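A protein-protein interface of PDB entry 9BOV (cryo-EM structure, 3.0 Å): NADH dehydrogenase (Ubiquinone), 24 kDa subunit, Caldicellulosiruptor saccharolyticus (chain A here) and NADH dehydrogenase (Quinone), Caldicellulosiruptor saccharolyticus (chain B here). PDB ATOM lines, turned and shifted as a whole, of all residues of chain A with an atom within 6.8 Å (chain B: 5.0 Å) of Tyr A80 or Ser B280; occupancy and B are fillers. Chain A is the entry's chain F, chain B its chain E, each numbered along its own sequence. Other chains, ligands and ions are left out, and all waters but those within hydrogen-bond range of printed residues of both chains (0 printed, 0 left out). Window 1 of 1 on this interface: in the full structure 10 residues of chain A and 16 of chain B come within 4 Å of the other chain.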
ATOM      1  N   SER A  38       8.129  22.751 -19.277  1.00  0.00           N
ATOM      2  CA  SER A  38       7.639  21.459 -19.735  1.00  0.00           C
ATOM      3  C   SER A  38       8.638  20.739 -20.631  1.00  0.00           C
ATOM      4  O   SER A  38       8.306  19.694 -21.197  1.00  0.00           O
ATOM      5  CB  SER A  38       6.310  21.631 -20.472  1.00  0.00           C
ATOM      6  OG  SER A  38       5.489  22.586 -19.823  1.00  0.00           O
ATOM      7  N   ILE A  41      12.619  17.081 -19.780  1.00  0.00           N
ATOM      8  CA  ILE A  41      13.126  15.787 -20.224  1.00  0.00           C
ATOM      9  C   ILE A  41      14.127  15.969 -21.356  1.00  0.00           C
ATOM     10  O   ILE A  41      15.150  15.276 -21.415  1.00  0.00           O
ATOM     11  CB  ILE A  41      11.965  14.865 -20.633  1.00  0.00           C
ATOM     12  CG1 ILE A  41      10.846  14.931 -19.594  1.00  0.00           C
ATOM     13  CG2 ILE A  41      12.456  13.436 -20.791  1.00  0.00           C
ATOM     14  CD1 ILE A  41       9.612  14.156 -19.978  1.00  0.00           C
ATOM     15  N   GLY A  75      13.169  13.137  -9.758  1.00  0.00           N
ATOM     16  CA  GLY A  75      12.179  12.134 -10.115  1.00  0.00           C
ATOM     17  C   GLY A  75      12.163  11.835 -11.602  1.00  0.00           C
ATOM     18  O   GLY A  75      12.166  10.672 -12.014  1.00  0.00           O
ATOM     19  N   ILE A  76      12.162  12.883 -12.430  1.00  0.00           N
ATOM     20  CA  ILE A  76      12.106  12.663 -13.872  1.00  0.00           C
ATOM     21  C   ILE A  76      13.400  12.005 -14.342  1.00  0.00           C
ATOM     22  O   ILE A  76      13.390  11.155 -15.240  1.00  0.00           O
ATOM     23  CB  ILE A  76      11.819  13.985 -14.616  1.00  0.00           C
ATOM     24  CG1 ILE A  76      11.973  13.836 -16.124  1.00  0.00           C
ATOM     25  CG2 ILE A  76      12.778  15.059 -14.215  1.00  0.00           C
ATOM     26  CD1 ILE A  76      11.143  12.736 -16.707  1.00  0.00           C
ATOM     27  N   ALA A  77      14.530  12.362 -13.723  1.00  0.00           N
ATOM     28  CA  ALA A  77      15.807  11.767 -14.104  1.00  0.00           C
ATOM     29  C   ALA A  77      15.850  10.283 -13.769  1.00  0.00           C
ATOM     30  O   ALA A  77      16.219   9.458 -14.612  1.00  0.00           O
ATOM     31  CB  ALA A  77      16.955  12.503 -13.415  1.00  0.00           C
ATOM     32  N   THR A  78      15.474   9.919 -12.544  1.00  0.00           N
ATOM     33  CA  THR A  78      15.561   8.526 -12.127  1.00  0.00           C
ATOM     34  C   THR A  78      14.398   7.677 -12.621  1.00  0.00           C
ATOM     35  O   THR A  78      14.440   6.453 -12.454  1.00  0.00           O
ATOM     36  CB  THR A  78      15.641   8.431 -10.603  1.00  0.00           C
ATOM     37  OG1 THR A  78      14.594   9.214 -10.015  1.00  0.00           O
ATOM     38  CG2 THR A  78      16.983   8.936 -10.115  1.00  0.00           C
ATOM     39  N   PHE A  79      13.367   8.285 -13.213  1.00  0.00           N
ATOM     40  CA  PHE A  79      12.253   7.495 -13.727  1.00  0.00           C
ATOM     41  C   PHE A  79      12.703   6.545 -14.830  1.00  0.00           C
ATOM     42  O   PHE A  79      12.297   5.378 -14.856  1.00  0.00           O
ATOM     43  CB  PHE A  79      11.147   8.419 -14.236  1.00  0.00           C
ATOM     44  CG  PHE A  79       9.920   7.691 -14.707  1.00  0.00           C
ATOM     45  CD1 PHE A  79       8.890   7.411 -13.831  1.00  0.00           C
ATOM     46  CD2 PHE A  79       9.794   7.295 -16.025  1.00  0.00           C
ATOM     47  CE1 PHE A  79       7.762   6.744 -14.258  1.00  0.00           C
ATOM     48  CE2 PHE A  79       8.668   6.626 -16.457  1.00  0.00           C
ATOM     49  CZ  PHE A  79       7.651   6.351 -15.572  1.00  0.00           C
ATOM     50  N   TYR A  80      13.540   7.021 -15.745  1.00  0.00           N
ATOM     51  CA  TYR A  80      13.931   6.237 -16.906  1.00  0.00           C
ATOM     52  C   TYR A  80      15.238   5.498 -16.660  1.00  0.00           C
ATOM     53  O   TYR A  80      16.107   5.956 -15.915  1.00  0.00           O
ATOM     54  CB  TYR A  80      14.069   7.132 -18.136  1.00  0.00           C
ATOM     55  CG  TYR A  80      12.811   7.888 -18.476  1.00  0.00           C
ATOM     56  CD1 TYR A  80      11.784   7.281 -19.181  1.00  0.00           C
ATOM     57  CD2 TYR A  80      12.646   9.205 -18.088  1.00  0.00           C
ATOM     58  CE1 TYR A  80      10.630   7.970 -19.493  1.00  0.00           C
ATOM     59  CE2 TYR A  80      11.497   9.897 -18.398  1.00  0.00           C
ATOM     60  CZ  TYR A  80      10.492   9.277 -19.097  1.00  0.00           C
ATOM     61  OH  TYR A  80       9.344   9.969 -19.403  1.00  0.00           O
ATOM     62  N   ALA A  81      15.365   4.335 -17.300  1.00  0.00           N
ATOM     63  CA  ALA A  81      16.589   3.552 -17.224  1.00  0.00           C
ATOM     64  C   ALA A  81      17.682   4.078 -18.141  1.00  0.00           C
ATOM     65  O   ALA A  81      18.833   3.645 -18.019  1.00  0.00           O
ATOM     66  CB  ALA A  81      16.299   2.087 -17.557  1.00  0.00           C
ATOM     67  N   GLN A  82      17.351   4.992 -19.055  1.00  0.00           N
ATOM     68  CA  GLN A  82      18.371   5.570 -19.922  1.00  0.00           C
ATOM     69  C   GLN A  82      19.243   6.564 -19.168  1.00  0.00           C
ATOM     70  O   GLN A  82      20.422   6.733 -19.503  1.00  0.00           O
ATOM     71  CB  GLN A  82      17.711   6.239 -21.127  1.00  0.00           C
ATOM     72  CG  GLN A  82      18.680   6.848 -22.121  1.00  0.00           C
ATOM     73  CD  GLN A  82      18.019   7.861 -23.029  1.00  0.00           C
ATOM     74  OE1 GLN A  82      16.997   8.450 -22.682  1.00  0.00           O
ATOM     75  NE2 GLN A  82      18.597   8.065 -24.207  1.00  0.00           N
ATOM     76  N   PHE A  83      18.694   7.218 -18.147  1.00  0.00           N
ATOM     77  CA  PHE A  83      19.447   8.174 -17.348  1.00  0.00           C
ATOM     78  C   PHE A  83      20.105   7.457 -16.177  1.00  0.00           C
ATOM     79  O   PHE A  83      19.413   6.915 -15.309  1.00  0.00           O
ATOM     80  CB  PHE A  83      18.533   9.281 -16.835  1.00  0.00           C
ATOM     81  CG  PHE A  83      17.770   9.993 -17.911  1.00  0.00           C
ATOM     82  CD1 PHE A  83      18.341  10.228 -19.145  1.00  0.00           C
ATOM     83  CD2 PHE A  83      16.482  10.436 -17.679  1.00  0.00           C
ATOM     84  CE1 PHE A  83      17.638  10.887 -20.130  1.00  0.00           C
ATOM     85  CE2 PHE A  83      15.775  11.094 -18.658  1.00  0.00           C
ATOM     86  CZ  PHE A  83      16.353  11.320 -19.885  1.00  0.00           C
ATOM     87  N   ARG A  84      21.434   7.462 -16.142  1.00  0.00           N
ATOM     88  CA  ARG A  84      22.180   6.893 -15.030  1.00  0.00           C
ATOM     89  C   ARG A  84      23.055   7.971 -14.410  1.00  0.00           C
ATOM     90  O   ARG A  84      23.690   8.755 -15.121  1.00  0.00           O
ATOM     91  CB  ARG A  84      23.015   5.685 -15.477  1.00  0.00           C
ATOM     92  CG  ARG A  84      24.119   5.971 -16.480  1.00  0.00           C
ATOM     93  CD  ARG A  84      25.249   4.970 -16.303  1.00  0.00           C
ATOM     94  NE  ARG A  84      26.352   5.193 -17.230  1.00  0.00           N
ATOM     95  CZ  ARG A  84      27.580   4.723 -17.057  1.00  0.00           C
ATOM     96  NH1 ARG A  84      27.900   4.005 -15.993  1.00  0.00           N
ATOM     97  NH2 ARG A  84      28.507   4.973 -17.977  1.00  0.00           N
ATOM     98  N   TYR B 222       4.649  12.218 -30.395  1.00  0.00           N
ATOM     99  CA  TYR B 222       5.496  11.662 -29.344  1.00  0.00           C
ATOM    100  C   TYR B 222       6.276  10.504 -29.945  1.00  0.00           C
ATOM    101  O   TYR B 222       5.820   9.361 -29.964  1.00  0.00           O
ATOM    102  CB  TYR B 222       4.661  11.214 -28.155  1.00  0.00           C
ATOM    103  CG  TYR B 222       5.460  10.928 -26.907  1.00  0.00           C
ATOM    104  CD1 TYR B 222       5.824  11.948 -26.043  1.00  0.00           C
ATOM    105  CD2 TYR B 222       5.860   9.637 -26.598  1.00  0.00           C
ATOM    106  CE1 TYR B 222       6.549  11.688 -24.903  1.00  0.00           C
ATOM    107  CE2 TYR B 222       6.584   9.369 -25.460  1.00  0.00           C
ATOM    108  CZ  TYR B 222       6.928  10.397 -24.617  1.00  0.00           C
ATOM    109  OH  TYR B 222       7.655  10.131 -23.482  1.00  0.00           O
ATOM    110  N   ALA B 266      12.080   9.954 -23.413  1.00  0.00           N
ATOM    111  CA  ALA B 266      13.327   9.368 -22.937  1.00  0.00           C
ATOM    112  C   ALA B 266      13.352   7.856 -23.092  1.00  0.00           C
ATOM    113  O   ALA B 266      14.434   7.263 -23.083  1.00  0.00           O
ATOM    114  CB  ALA B 266      13.561   9.745 -21.475  1.00  0.00           C
ATOM    115  N   GLY B 267      12.192   7.224 -23.234  1.00  0.00           N
ATOM    116  CA  GLY B 267      12.127   5.791 -23.432  1.00  0.00           C
ATOM    117  C   GLY B 267      11.634   5.042 -22.214  1.00  0.00           C
ATOM    118  O   GLY B 267      12.396   4.792 -21.275  1.00  0.00           O
ATOM    119  N   ALA B 268      10.355   4.675 -22.223  1.00  0.00           N
ATOM    120  CA  ALA B 268       9.765   3.894 -21.148  1.00  0.00           C
ATOM    121  C   ALA B 268       8.507   3.226 -21.678  1.00  0.00           C
ATOM    122  O   ALA B 268       7.771   3.820 -22.468  1.00  0.00           O
ATOM    123  CB  ALA B 268       9.435   4.762 -19.931  1.00  0.00           C
ATOM    124  N   CYS B 271       5.382   5.104 -20.564  1.00  0.00           N
ATOM    125  CA  CYS B 271       5.174   6.413 -21.171  1.00  0.00           C
ATOM    126  C   CYS B 271       4.368   6.323 -22.457  1.00  0.00           C
ATOM    127  O   CYS B 271       3.855   7.345 -22.924  1.00  0.00           O
ATOM    128  CB  CYS B 271       6.514   7.096 -21.439  1.00  0.00           C
ATOM    129  SG  CYS B 271       7.118   8.102 -20.065  1.00  0.00           S
ATOM    130  N   ALA B 276       0.048   8.673 -19.223  1.00  0.00           N
ATOM    131  CA  ALA B 276       1.458   8.864 -18.915  1.00  0.00           C
ATOM    132  C   ALA B 276       2.158   9.648 -20.011  1.00  0.00           C
ATOM    133  O   ALA B 276       3.081  10.417 -19.729  1.00  0.00           O
ATOM    134  CB  ALA B 276       2.144   7.519 -18.704  1.00  0.00           C
ATOM    135  N   LEU B 277       1.734   9.469 -21.262  1.00  0.00           N
ATOM    136  CA  LEU B 277       2.253  10.294 -22.346  1.00  0.00           C
ATOM    137  C   LEU B 277       1.876  11.754 -22.153  1.00  0.00           C
ATOM    138  O   LEU B 277       2.683  12.653 -22.414  1.00  0.00           O
ATOM    139  CB  LEU B 277       1.734   9.783 -23.684  1.00  0.00           C
ATOM    140  CG  LEU B 277       2.297  10.477 -24.913  1.00  0.00           C
ATOM    141  CD1 LEU B 277       2.576   9.447 -25.945  1.00  0.00           C
ATOM    142  CD2 LEU B 277       1.306  11.483 -25.454  1.00  0.00           C
ATOM    143  N   ILE B 278       0.642  12.008 -21.715  1.00  0.00           N
ATOM    144  CA  ILE B 278       0.219  13.377 -21.433  1.00  0.00           C
ATOM    145  C   ILE B 278       1.089  13.980 -20.339  1.00  0.00           C
ATOM    146  O   ILE B 278       1.528  15.133 -20.435  1.00  0.00           O
ATOM    147  CB  ILE B 278      -1.274  13.398 -21.060  1.00  0.00           C
ATOM    148  CG1 ILE B 278      -2.128  13.337 -22.323  1.00  0.00           C
ATOM    149  CG2 ILE B 278      -1.612  14.627 -20.237  1.00  0.00           C
ATOM    150  CD1 ILE B 278      -3.418  12.593 -22.143  1.00  0.00           C
ATOM    151  N   ALA B 279       1.365  13.204 -19.291  1.00  0.00           N
ATOM    152  CA  ALA B 279       2.230  13.689 -18.220  1.00  0.00           C
ATOM    153  C   ALA B 279       3.647  13.953 -18.720  1.00  0.00           C
ATOM    154  O   ALA B 279       4.262  14.962 -18.355  1.00  0.00           O
ATOM    155  CB  ALA B 279       2.249  12.689 -17.065  1.00  0.00           C
ATOM    156  N   SER B 280       4.182  13.057 -19.553  1.00  0.00           N
ATOM    157  CA  SER B 280       5.539  13.233 -20.065  1.00  0.00           C
ATOM    158  C   SER B 280       5.645  14.469 -20.948  1.00  0.00           C
ATOM    159  O   SER B 280       6.630  15.212 -20.873  1.00  0.00           O
ATOM    160  CB  SER B 280       5.975  11.988 -20.833  1.00  0.00           C
ATOM    161  OG  SER B 280       6.035  10.858 -19.981  1.00  0.00           O
ATOM    162  N   ILE B 281       4.644  14.702 -21.799  1.00  0.00           N
ATOM    163  CA  ILE B 281       4.623  15.923 -22.600  1.00  0.00           C
ATOM    164  C   ILE B 281       4.509  17.144 -21.697  1.00  0.00           C
ATOM    165  O   ILE B 281       5.134  18.181 -21.947  1.00  0.00           O
ATOM    166  CB  ILE B 281       3.483  15.867 -23.633  1.00  0.00           C
ATOM    167  CG1 ILE B 281       3.811  14.852 -24.728  1.00  0.00           C
ATOM    168  CG2 ILE B 281       3.231  17.237 -24.233  1.00  0.00           C
ATOM    169  CD1 ILE B 281       2.804  14.821 -25.847  1.00  0.00           C
ATOM    170  N   GLU B 282       3.722  17.034 -20.624  1.00  0.00           N
ATOM    171  CA  GLU B 282       3.615  18.125 -19.665  1.00  0.00           C
ATOM    172  C   GLU B 282       4.923  18.378 -18.928  1.00  0.00           C
ATOM    173  O   GLU B 282       5.068  19.427 -18.292  1.00  0.00           O
ATOM    174  CB  GLU B 282       2.505  17.832 -18.658  1.00  0.00           C
ATOM    175  CG  GLU B 282       1.113  18.163 -19.156  1.00  0.00           C
ATOM    176  CD  GLU B 282       0.055  17.958 -18.094  1.00  0.00           C
ATOM    177  OE1 GLU B 282       0.425  17.755 -16.918  1.00  0.00           O
ATOM    178  OE2 GLU B 282      -1.146  17.992 -18.433  1.00  0.00           O
ATOM    179  N   GLY B 283       5.868  17.450 -18.993  1.00  0.00           N
ATOM    180  CA  GLY B 283       7.163  17.626 -18.384  1.00  0.00           C
ATOM    181  C   GLY B 283       7.358  16.985 -17.030  1.00  0.00           C
ATOM    182  O   GLY B 283       8.255  17.406 -16.292  1.00  0.00           O
ATOM    183  N   GLU B 284       6.558  15.990 -16.677  1.00  0.00           N
ATOM    184  CA  GLU B 284       6.703  15.260 -15.428  1.00  0.00           C
ATOM    185  C   GLU B 284       7.034  13.804 -15.733  1.00  0.00           C
ATOM    186  O   GLU B 284       7.164  13.403 -16.891  1.00  0.00           O
ATOM    187  CB  GLU B 284       5.432  15.364 -14.583  1.00  0.00           C
ATOM    188  CG  GLU B 284       4.838  16.759 -14.525  1.00  0.00           C
ATOM    189  CD  GLU B 284       3.370  16.751 -14.149  1.00  0.00           C
ATOM    190  OE1 GLU B 284       2.801  15.650 -13.996  1.00  0.00           O
ATOM    191  OE2 GLU B 284       2.785  17.844 -14.008  1.00  0.00           O
ATOM    192  N   ARG B 285       7.170  13.007 -14.678  1.00  0.00           N
ATOM    193  CA  ARG B 285       7.425  11.587 -14.860  1.00  0.00           C
ATOM    194  C   ARG B 285       6.172  10.889 -15.369  1.00  0.00           C
ATOM    195  O   ARG B 285       5.047  11.349 -15.158  1.00  0.00           O
ATOM    196  CB  ARG B 285       7.898  10.950 -13.554  1.00  0.00           C
ATOM    197  CG  ARG B 285       7.053  11.294 -12.350  1.00  0.00           C
ATOM    198  CD  ARG B 285       7.654  10.724 -11.078  1.00  0.00           C
ATOM    199  NE  ARG B 285       7.947   9.301 -11.186  1.00  0.00           N
ATOM    200  CZ  ARG B 285       8.956   8.697 -10.574  1.00  0.00           C
ATOM    201  NH1 ARG B 285       9.811   9.371  -9.823  1.00  0.00           N
ATOM    202  NH2 ARG B 285       9.111   7.384 -10.716  1.00  0.00           N
ATOM    203  N   GLY B 286       6.376   9.766 -16.049  1.00  0.00           N
ATOM    204  CA  GLY B 286       5.282   9.067 -16.689  1.00  0.00           C
ATOM    205  C   GLY B 286       4.478   8.191 -15.751  1.00  0.00           C
ATOM    206  O   GLY B 286       4.584   6.964 -15.794  1.00  0.00           O
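The side-chain hydroxyl (OH) of Tyr A80 is in hydrogen-bond range of the side-chain sulfur (SG) of Cys B271, at 3.0 Å.
The side-chain hydroxyl (OG) of Ser B280 sits at hydrogen-bond distance from the side-chain hydroxyl (OH) of Tyr A80 (3.5 Å).
O of Ala B266 sits close to OE1 of Gln A82.
NH1 of Arg B285 is in hydrogen-bond range of O of Gly A75 (3.5 Å).
The backbone carbonyl oxygen (O) of Gly A75 lies within hydrogen-bond range of the side-chain hydroxyl (OG1) of Thr A78.
The backbone carbonyl oxygen (O) of Cys B271 lies close to the backbone NH (N) of Leu B277 (3.4 Å).
The side-chain sulfur (SG) of Cys B271 sits at hydrogen-bond distance from the side-chain hydroxyl (OG) of Ser B280.
O of Ala B276 is in hydrogen-bond range of OG of Ser B280.
CB of Ser A38 touches O of Glu B282, 3.3 Å away.
O of Ser A38 touches CA of Gly B283, 3.7 Å away.
Ile A41 touches Ala B266.
Ile A41 touches Ser B280 (CD1 to O, 3.3 Å).
CD1 of Phe A79 touches NH2 of Arg B285 (3.1 Å).
Phe A79 touches Gly B286.
Tyr A80 touches Ala B266.
CD1 of Tyr A80 touches O of Gly B267 (3.3 Å).
Tyr A80 touches Ala B268.
Ala B266 touches Phe A83.
Ser B280 touches just these residues of chain A: Ile A41 (3.3 Å) and Tyr A80 (3.5 Å).
Printed residues of chain A within 4 Å of Cys B271: Tyr A80 (3.0 Å).
Printed residues of chain A within 4 Å of Arg B285: Gly A75 (3.5 Å) and Phe A79 (3.1 Å).
Of the printed residues of chain B, Ile A41 touches Ala B266 (3.9 Å) and Ser B280 (3.3 Å).
Of the printed residues of chain A, Gly B267 touches Tyr A80.
Of the printed residues of chain B, Ser A38 touches Ile B281 (3.6 Å), Glu B282 (3.3 Å) and Gly B283 (3.7 Å).
The nearest residue of chain B that does not touch Tyr A80 is Tyr B222 (4.4 Å).
The nearest printed residue of chain B that does not touch Ile A41 is Glu B284 (4.01 Å).
Printed residues of chain A that touch a printed residue of chain B: Ser A38, Ile A41, Gly A75, Phe A79, Tyr A80, Gln A82 and Phe A83.
Hydrophobic or aromatic side chains of chain A within 4 Å of the printed part of chain B: Ile A41, Phe A79, Tyr A80 and Phe A83.
Among the printed residues, no Asp or Glu carboxylate lies within 4 Å of a Lys or Arg side-chain nitrogen of the other chain.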
